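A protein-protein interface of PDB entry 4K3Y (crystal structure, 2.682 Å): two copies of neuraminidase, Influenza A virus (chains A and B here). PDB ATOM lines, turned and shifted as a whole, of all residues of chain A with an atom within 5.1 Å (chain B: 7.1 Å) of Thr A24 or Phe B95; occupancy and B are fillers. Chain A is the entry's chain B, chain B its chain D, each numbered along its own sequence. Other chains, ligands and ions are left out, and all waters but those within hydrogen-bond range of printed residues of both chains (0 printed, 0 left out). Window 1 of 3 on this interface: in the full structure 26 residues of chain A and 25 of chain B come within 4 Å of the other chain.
No position is printed for both chains.
Hydrophobic or aromatic side chains of chain B within 4 Å of the printed part of chain A: Phe B95, Val B98, Leu B125 and Ile B130. Of the 10 printed residues of chain A, 7 touch a printed residue of chain B. Hydrophobic or aromatic side chains of chain A within 4 Å of the printed part of chain B: Val A22, Pro A23 and Tyr A25. Among the printed residues, 14 pairs touch across the chains.
Among the printed residues, pairs that only touch across the chains: Thr A24 with Gly B128, Arg A26 with Val B98, Thr A24 with Phe B95, Arg A26 with Phe B95, Tyr A25 with Phe B95, Val A22 with Ile B130, Gly A85 with Lys B94, Pro A23 with Val B98, Thr A24 with Leu B125, Cys A357 with Ile B130 and Gly A85 with Leu B93.
Thr A24 touches just these residues of chain B: Phe B95 (3.4 Å), Leu B125 (3.8 Å) and Gly B128 (3.2 Å). Of the printed residues of chain A, Phe B95 touches Thr A24 (3.4 Å), Tyr A25 (3.6 Å), Arg A26 (3.4 Å) and Gly A85 (3.0 Å). Of the printed residues of chain B, Val A22 touches Ile B130 (3.6 Å). Of the printed residues of chain B, Tyr A25 touches Phe B95. Of the printed residues of chain B, Cys A357 touches Ile B130 (3.9 Å). Printed residues of chain A within 4 Å of Lys B94: Gly A85 (3.6 Å). Printed residues of chain A within 4 Å of Leu B93: Gly A85. The nearest residue of chain B that does not touch Thr A24 is Ile B130 (4.2 Å). The nearest printed residue of chain A that does not touch Phe B95 is Pro A23 (5.5 Å).
O of Gly A85 lies within hydrogen-bond range of N of Phe B95 (3.0 Å). The guanidinium group of Arg A26 lies within hydrogen-bond range of the backbone carbonyl oxygen of Met B77 (3.3 Å). NH2 of Arg A26 lies within hydrogen-bond range of OD1 of Asn B78 (2.7 Å).
The backbone NH of Asn B78 lies within hydrogen-bond range of the backbone carbonyl oxygen of Gly B99 (3.5 Å). The backbone carbonyl oxygen of Thr A355 is in hydrogen-bond range of the backbone NH of Thr A24 (2.9 Å). O of Val A22 sits at hydrogen-bond distance from N of Cys A357. O of Tyr A25 lies within hydrogen-bond range of N of Thr A355 (2.8 Å). O of Met B77 is in hydrogen-bond range of N of Gly B99, at 3.0 Å. The side-chain hydroxyl (OG1) of Thr A24 lies within hydrogen-bond range of the side-chain sulfur (SG) of Cys A357, 3.6 Å away.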
ATOM      1  N   VAL A  22      -9.516 -21.083   9.445  1.00  0.00           N
ATOM      2  CA  VAL A  22     -10.628 -22.031   9.388  1.00  0.00           C
ATOM      3  C   VAL A  22     -11.934 -21.294   9.632  1.00  0.00           C
ATOM      4  O   VAL A  22     -12.024 -20.458  10.544  1.00  0.00           O
ATOM      5  CB  VAL A  22     -10.486 -23.143  10.438  1.00  0.00           C
ATOM      6  CG1 VAL A  22     -11.714 -24.052  10.414  1.00  0.00           C
ATOM      7  CG2 VAL A  22      -9.212 -23.943  10.202  1.00  0.00           C
ATOM      8  N   PRO A  23     -12.949 -21.586   8.806  1.00  0.00           N
ATOM      9  CA  PRO A  23     -14.276 -20.970   8.963  1.00  0.00           C
ATOM     10  C   PRO A  23     -14.986 -21.359  10.264  1.00  0.00           C
ATOM     11  O   PRO A  23     -14.946 -22.519  10.689  1.00  0.00           O
ATOM     12  CB  PRO A  23     -15.056 -21.479   7.741  1.00  0.00           C
ATOM     13  CG  PRO A  23     -14.330 -22.683   7.299  1.00  0.00           C
ATOM     14  CD  PRO A  23     -12.878 -22.443   7.612  1.00  0.00           C
ATOM     15  N   THR A  24     -15.629 -20.381  10.894  1.00  0.00           N
ATOM     16  CA  THR A  24     -16.348 -20.624  12.138  1.00  0.00           C
ATOM     17  C   THR A  24     -17.846 -20.333  11.984  1.00  0.00           C
ATOM     18  O   THR A  24     -18.685 -20.839  12.743  1.00  0.00           O
ATOM     19  CB  THR A  24     -15.769 -19.796  13.287  1.00  0.00           C
ATOM     20  OG1 THR A  24     -15.461 -18.481  12.818  1.00  0.00           O
ATOM     21  CG2 THR A  24     -14.507 -20.442  13.812  1.00  0.00           C
ATOM     22  N   TYR A  25     -18.172 -19.508  11.001  1.00  0.00           N
ATOM     23  CA  TYR A  25     -19.543 -19.392  10.568  1.00  0.00           C
ATOM     24  C   TYR A  25     -19.531 -19.308   9.066  1.00  0.00           C
ATOM     25  O   TYR A  25     -18.683 -18.623   8.477  1.00  0.00           O
ATOM     26  CB  TYR A  25     -20.239 -18.151  11.150  1.00  0.00           C
ATOM     27  CG  TYR A  25     -21.654 -17.967  10.628  1.00  0.00           C
ATOM     28  CD1 TYR A  25     -22.691 -18.797  11.057  1.00  0.00           C
ATOM     29  CD2 TYR A  25     -21.950 -16.977   9.699  1.00  0.00           C
ATOM     30  CE1 TYR A  25     -23.975 -18.636  10.589  1.00  0.00           C
ATOM     31  CE2 TYR A  25     -23.248 -16.811   9.222  1.00  0.00           C
ATOM     32  CZ  TYR A  25     -24.254 -17.643   9.672  1.00  0.00           C
ATOM     33  OH  TYR A  25     -25.547 -17.477   9.208  1.00  0.00           O
ATOM     34  N   ARG A  26     -20.481 -20.000   8.450  1.00  0.00           N
ATOM     35  CA  ARG A  26     -20.634 -19.946   7.012  1.00  0.00           C
ATOM     36  C   ARG A  26     -22.118 -19.873   6.710  1.00  0.00           C
ATOM     37  O   ARG A  26     -22.852 -20.832   6.945  1.00  0.00           O
ATOM     38  CB  ARG A  26     -19.989 -21.168   6.359  1.00  0.00           C
ATOM     39  CG  ARG A  26     -19.896 -21.078   4.856  1.00  0.00           C
ATOM     40  CD  ARG A  26     -19.034 -22.185   4.292  1.00  0.00           C
ATOM     41  NE  ARG A  26     -19.686 -23.486   4.369  1.00  0.00           N
ATOM     42  CZ  ARG A  26     -19.173 -24.608   3.877  1.00  0.00           C
ATOM     43  NH1 ARG A  26     -17.989 -24.595   3.280  1.00  0.00           N
ATOM     44  NH2 ARG A  26     -19.845 -25.744   3.987  1.00  0.00           N
ATOM     45  N   GLY A  85     -24.037 -17.252  14.434  1.00  0.00           N
ATOM     46  CA  GLY A  85     -24.381 -18.665  14.403  1.00  0.00           C
ATOM     47  C   GLY A  85     -25.877 -18.894  14.341  1.00  0.00           C
ATOM     48  O   GLY A  85     -26.345 -19.935  13.871  1.00  0.00           O
ATOM     49  N   TYR A 322     -12.236  -8.980  13.536  1.00  0.00           N
ATOM     50  CA  TYR A 322     -12.780  -8.981  14.898  1.00  0.00           C
ATOM     51  C   TYR A 322     -11.973  -9.873  15.834  1.00  0.00           C
ATOM     52  O   TYR A 322     -11.316 -10.819  15.391  1.00  0.00           O
ATOM     53  CB  TYR A 322     -14.270  -9.370  14.929  1.00  0.00           C
ATOM     54  CG  TYR A 322     -14.593 -10.800  14.541  1.00  0.00           C
ATOM     55  CD1 TYR A 322     -14.846 -11.135  13.214  1.00  0.00           C
ATOM     56  CD2 TYR A 322     -14.672 -11.805  15.499  1.00  0.00           C
ATOM     57  CE1 TYR A 322     -15.152 -12.429  12.848  1.00  0.00           C
ATOM     58  CE2 TYR A 322     -14.989 -13.111  15.142  1.00  0.00           C
ATOM     59  CZ  TYR A 322     -15.230 -13.410  13.810  1.00  0.00           C
ATOM     60  OH  TYR A 322     -15.544 -14.691  13.428  1.00  0.00           O
ATOM     61  N   THR A 355     -17.131 -16.341   8.234  1.00  0.00           N
ATOM     62  CA  THR A 355     -16.097 -15.885   9.165  1.00  0.00           C
ATOM     63  C   THR A 355     -14.947 -16.890   9.209  1.00  0.00           C
ATOM     64  O   THR A 355     -15.173 -18.098   9.155  1.00  0.00           O
ATOM     65  CB  THR A 355     -16.633 -15.642  10.600  1.00  0.00           C
ATOM     66  OG1 THR A 355     -17.309 -16.814  11.067  1.00  0.00           O
ATOM     67  CG2 THR A 355     -17.592 -14.449  10.637  1.00  0.00           C
ATOM     68  N   PHE A 356     -13.722 -16.378   9.288  1.00  0.00           N
ATOM     69  CA  PHE A 356     -12.530 -17.209   9.425  1.00  0.00           C
ATOM     70  C   PHE A 356     -11.782 -16.823  10.708  1.00  0.00           C
ATOM     71  O   PHE A 356     -11.625 -15.622  11.006  1.00  0.00           O
ATOM     72  CB  PHE A 356     -11.595 -17.013   8.221  1.00  0.00           C
ATOM     73  CG  PHE A 356     -12.047 -17.714   6.975  1.00  0.00           C
ATOM     74  CD1 PHE A 356     -11.750 -19.056   6.778  1.00  0.00           C
ATOM     75  CD2 PHE A 356     -12.764 -17.037   5.996  1.00  0.00           C
ATOM     76  CE1 PHE A 356     -12.163 -19.718   5.631  1.00  0.00           C
ATOM     77  CE2 PHE A 356     -13.181 -17.697   4.845  1.00  0.00           C
ATOM     78  CZ  PHE A 356     -12.877 -19.041   4.662  1.00  0.00           C
ATOM     79  N   CYS A 357     -11.331 -17.826  11.468  1.00  0.00           N
ATOM     80  CA  CYS A 357     -10.448 -17.588  12.623  1.00  0.00           C
ATOM     81  C   CYS A 357      -9.059 -18.198  12.424  1.00  0.00           C
ATOM     82  O   CYS A 357      -8.918 -19.246  11.776  1.00  0.00           O
ATOM     83  CB  CYS A 357     -11.076 -18.106  13.925  1.00  0.00           C
ATOM     84  SG  CYS A 357     -12.569 -17.179  14.470  1.00  0.00           S
ATOM     85  N   MET B  77     -21.269 -29.319   3.043  1.00  0.00           N
ATOM     86  CA  MET B  77     -21.744 -29.872   4.312  1.00  0.00           C
ATOM     87  C   MET B  77     -21.360 -28.997   5.507  1.00  0.00           C
ATOM     88  O   MET B  77     -20.220 -28.539   5.623  1.00  0.00           O
ATOM     89  CB  MET B  77     -21.208 -31.299   4.526  1.00  0.00           C
ATOM     90  CG  MET B  77     -21.769 -32.397   3.606  1.00  0.00           C
ATOM     91  SD  MET B  77     -23.466 -32.877   3.972  1.00  0.00           S
ATOM     92  CE  MET B  77     -23.516 -34.538   3.311  1.00  0.00           C
ATOM     93  N   ASN B  78     -22.322 -28.771   6.395  1.00  0.00           N
ATOM     94  CA  ASN B  78     -22.075 -28.041   7.635  1.00  0.00           C
ATOM     95  C   ASN B  78     -22.510 -28.865   8.835  1.00  0.00           C
ATOM     96  O   ASN B  78     -23.294 -29.803   8.695  1.00  0.00           O
ATOM     97  CB  ASN B  78     -22.828 -26.705   7.642  1.00  0.00           C
ATOM     98  CG  ASN B  78     -22.309 -25.737   6.600  1.00  0.00           C
ATOM     99  OD1 ASN B  78     -21.096 -25.590   6.422  1.00  0.00           O
ATOM    100  ND2 ASN B  78     -23.223 -25.066   5.903  1.00  0.00           N
ATOM    101  N   VAL B  79     -21.997 -28.521  10.014  1.00  0.00           N
ATOM    102  CA  VAL B  79     -22.505 -29.094  11.256  1.00  0.00           C
ATOM    103  C   VAL B  79     -23.462 -28.120  11.939  1.00  0.00           C
ATOM    104  O   VAL B  79     -23.135 -26.946  12.134  1.00  0.00           O
ATOM    105  CB  VAL B  79     -21.376 -29.453  12.230  1.00  0.00           C
ATOM    106  CG1 VAL B  79     -21.845 -30.550  13.179  1.00  0.00           C
ATOM    107  CG2 VAL B  79     -20.150 -29.909  11.456  1.00  0.00           C
ATOM    108  N   TYR B  80     -24.649 -28.607  12.287  1.00  0.00           N
ATOM    109  CA  TYR B  80     -25.624 -27.808  13.028  1.00  0.00           C
ATOM    110  C   TYR B  80     -26.058 -28.521  14.304  1.00  0.00           C
ATOM    111  O   TYR B  80     -25.770 -29.702  14.503  1.00  0.00           O
ATOM    112  CB  TYR B  80     -26.868 -27.570  12.182  1.00  0.00           C
ATOM    113  CG  TYR B  80     -26.632 -26.954  10.827  1.00  0.00           C
ATOM    114  CD1 TYR B  80     -26.365 -27.753   9.712  1.00  0.00           C
ATOM    115  CD2 TYR B  80     -26.714 -25.574  10.647  1.00  0.00           C
ATOM    116  CE1 TYR B  80     -26.166 -27.183   8.452  1.00  0.00           C
ATOM    117  CE2 TYR B  80     -26.518 -24.995   9.396  1.00  0.00           C
ATOM    118  CZ  TYR B  80     -26.241 -25.800   8.304  1.00  0.00           C
ATOM    119  OH  TYR B  80     -26.042 -25.218   7.068  1.00  0.00           O
ATOM    120  N   SER B  81     -26.769 -27.803  15.162  1.00  0.00           N
ATOM    121  CA  SER B  81     -27.442 -28.436  16.296  1.00  0.00           C
ATOM    122  C   SER B  81     -28.726 -27.697  16.688  1.00  0.00           C
ATOM    123  O   SER B  81     -28.897 -26.502  16.395  1.00  0.00           O
ATOM    124  CB  SER B  81     -26.506 -28.561  17.505  1.00  0.00           C
ATOM    125  OG  SER B  81     -26.272 -27.300  18.116  1.00  0.00           O
ATOM    126  N   LEU B  93     -32.118 -23.469  14.103  1.00  0.00           N
ATOM    127  CA  LEU B  93     -30.776 -23.949  13.825  1.00  0.00           C
ATOM    128  C   LEU B  93     -29.669 -23.098  14.456  1.00  0.00           C
ATOM    129  O   LEU B  93     -29.765 -21.865  14.542  1.00  0.00           O
ATOM    130  CB  LEU B  93     -30.560 -23.983  12.314  1.00  0.00           C
ATOM    131  CG  LEU B  93     -30.634 -25.344  11.634  1.00  0.00           C
ATOM    132  CD1 LEU B  93     -31.525 -26.292  12.408  1.00  0.00           C
ATOM    133  CD2 LEU B  93     -31.156 -25.159  10.229  1.00  0.00           C
ATOM    134  N   LYS B  94     -28.620 -23.778  14.906  1.00  0.00           N
ATOM    135  CA  LYS B  94     -27.370 -23.126  15.273  1.00  0.00           C
ATOM    136  C   LYS B  94     -26.239 -23.716  14.426  1.00  0.00           C
ATOM    137  O   LYS B  94     -25.977 -24.926  14.479  1.00  0.00           O
ATOM    138  CB  LYS B  94     -27.059 -23.324  16.758  1.00  0.00           C
ATOM    139  CG  LYS B  94     -25.639 -22.974  17.119  1.00  0.00           C
ATOM    140  CD  LYS B  94     -25.362 -23.232  18.583  1.00  0.00           C
ATOM    141  CE  LYS B  94     -24.086 -22.510  19.001  1.00  0.00           C
ATOM    142  NZ  LYS B  94     -23.949 -22.424  20.478  1.00  0.00           N
ATOM    143  N   PHE B  95     -25.589 -22.868  13.631  1.00  0.00           N
ATOM    144  CA  PHE B  95     -24.400 -23.281  12.895  1.00  0.00           C
ATOM    145  C   PHE B  95     -23.321 -23.713  13.889  1.00  0.00           C
ATOM    146  O   PHE B  95     -23.092 -23.036  14.895  1.00  0.00           O
ATOM    147  CB  PHE B  95     -23.867 -22.143  12.029  1.00  0.00           C
ATOM    148  CG  PHE B  95     -22.762 -22.560  11.110  1.00  0.00           C
ATOM    149  CD1 PHE B  95     -23.056 -23.065   9.850  1.00  0.00           C
ATOM    150  CD2 PHE B  95     -21.427 -22.470  11.506  1.00  0.00           C
ATOM    151  CE1 PHE B  95     -22.048 -23.462   8.994  1.00  0.00           C
ATOM    152  CE2 PHE B  95     -20.407 -22.869  10.656  1.00  0.00           C
ATOM    153  CZ  PHE B  95     -20.721 -23.364   9.394  1.00  0.00           C
ATOM    154  N   GLU B  96     -22.668 -24.839  13.617  1.00  0.00           N
ATOM    155  CA  GLU B  96     -21.662 -25.355  14.539  1.00  0.00           C
ATOM    156  C   GLU B  96     -20.246 -25.394  13.945  1.00  0.00           C
ATOM    157  O   GLU B  96     -19.290 -24.974  14.602  1.00  0.00           O
ATOM    158  CB  GLU B  96     -22.091 -26.719  15.095  1.00  0.00           C
ATOM    159  CG  GLU B  96     -23.274 -26.650  16.058  1.00  0.00           C
ATOM    160  CD  GLU B  96     -22.884 -26.111  17.432  1.00  0.00           C
ATOM    161  OE1 GLU B  96     -21.673 -25.892  17.675  1.00  0.00           O
ATOM    162  OE2 GLU B  96     -23.787 -25.913  18.273  1.00  0.00           O
ATOM    163  N   ALA B  97     -20.122 -25.887  12.711  1.00  0.00           N
ATOM    164  CA  ALA B  97     -18.836 -25.964  12.014  1.00  0.00           C
ATOM    165  C   ALA B  97     -19.081 -26.325  10.561  1.00  0.00           C
ATOM    166  O   ALA B  97     -20.194 -26.699  10.193  1.00  0.00           O
ATOM    167  CB  ALA B  97     -17.905 -27.010  12.665  1.00  0.00           C
ATOM    168  N   VAL B  98     -18.037 -26.224   9.745  1.00  0.00           N
ATOM    169  CA  VAL B  98     -18.058 -26.755   8.382  1.00  0.00           C
ATOM    170  C   VAL B  98     -17.556 -28.204   8.437  1.00  0.00           C
ATOM    171  O   VAL B  98     -16.531 -28.475   9.067  1.00  0.00           O
ATOM    172  CB  VAL B  98     -17.142 -25.907   7.462  1.00  0.00           C
ATOM    173  CG1 VAL B  98     -17.188 -26.388   6.016  1.00  0.00           C
ATOM    174  CG2 VAL B  98     -17.530 -24.436   7.549  1.00  0.00           C
ATOM    175  N   GLY B  99     -18.279 -29.137   7.813  1.00  0.00           N
ATOM    176  CA  GLY B  99     -17.882 -30.541   7.852  1.00  0.00           C
ATOM    177  C   GLY B  99     -18.934 -31.600   7.518  1.00  0.00           C
ATOM    178  O   GLY B  99     -20.121 -31.297   7.365  1.00  0.00           O
ATOM    179  N   LEU B 125     -13.504 -26.805  17.521  1.00  0.00           N
ATOM    180  CA  LEU B 125     -14.098 -25.514  17.892  1.00  0.00           C
ATOM    181  C   LEU B 125     -14.560 -25.498  19.340  1.00  0.00           C
ATOM    182  O   LEU B 125     -15.206 -26.442  19.807  1.00  0.00           O
ATOM    183  CB  LEU B 125     -15.244 -25.132  16.946  1.00  0.00           C
ATOM    184  CG  LEU B 125     -14.866 -24.869  15.478  1.00  0.00           C
ATOM    185  CD1 LEU B 125     -14.799 -26.170  14.697  1.00  0.00           C
ATOM    186  CD2 LEU B 125     -15.814 -23.885  14.796  1.00  0.00           C
ATOM    187  N   GLY B 128     -17.407 -20.925  19.558  1.00  0.00           N
ATOM    188  CA  GLY B 128     -17.333 -21.070  18.122  1.00  0.00           C
ATOM    189  C   GLY B 128     -15.992 -20.573  17.642  1.00  0.00           C
ATOM    190  O   GLY B 128     -15.907 -19.924  16.598  1.00  0.00           O
ATOM    191  N   ILE B 129     -14.945 -20.850  18.417  1.00  0.00           N
ATOM    192  CA  ILE B 129     -13.593 -20.450  18.028  1.00  0.00           C
ATOM    193  C   ILE B 129     -12.697 -21.669  17.855  1.00  0.00           C
ATOM    194  O   ILE B 129     -12.756 -22.627  18.633  1.00  0.00           O
ATOM    195  CB  ILE B 129     -12.980 -19.415  18.998  1.00  0.00           C
ATOM    196  CG1 ILE B 129     -12.136 -20.080  20.086  1.00  0.00           C
ATOM    197  CG2 ILE B 129     -14.073 -18.561  19.605  1.00  0.00           C
ATOM    198  CD1 ILE B 129     -11.421 -19.102  21.012  1.00  0.00           C
ATOM    199  N   ILE B 130     -11.893 -21.655  16.804  1.00  0.00           N
ATOM    200  CA  ILE B 130     -11.022 -22.785  16.550  1.00  0.00           C
ATOM    201  C   ILE B 130      -9.810 -22.811  17.500  1.00  0.00           C
ATOM    202  O   ILE B 130      -9.057 -21.830  17.618  1.00  0.00           O
ATOM    203  CB  ILE B 130     -10.625 -22.868  15.075  1.00  0.00           C
ATOM    204  CG1 ILE B 130      -9.877 -24.161  14.827  1.00  0.00           C
ATOM    205  CG2 ILE B 130      -9.799 -21.670  14.655  1.00  0.00           C
ATOM    206  CD1 ILE B 130     -10.375 -24.889  13.633  1.00  0.00           C
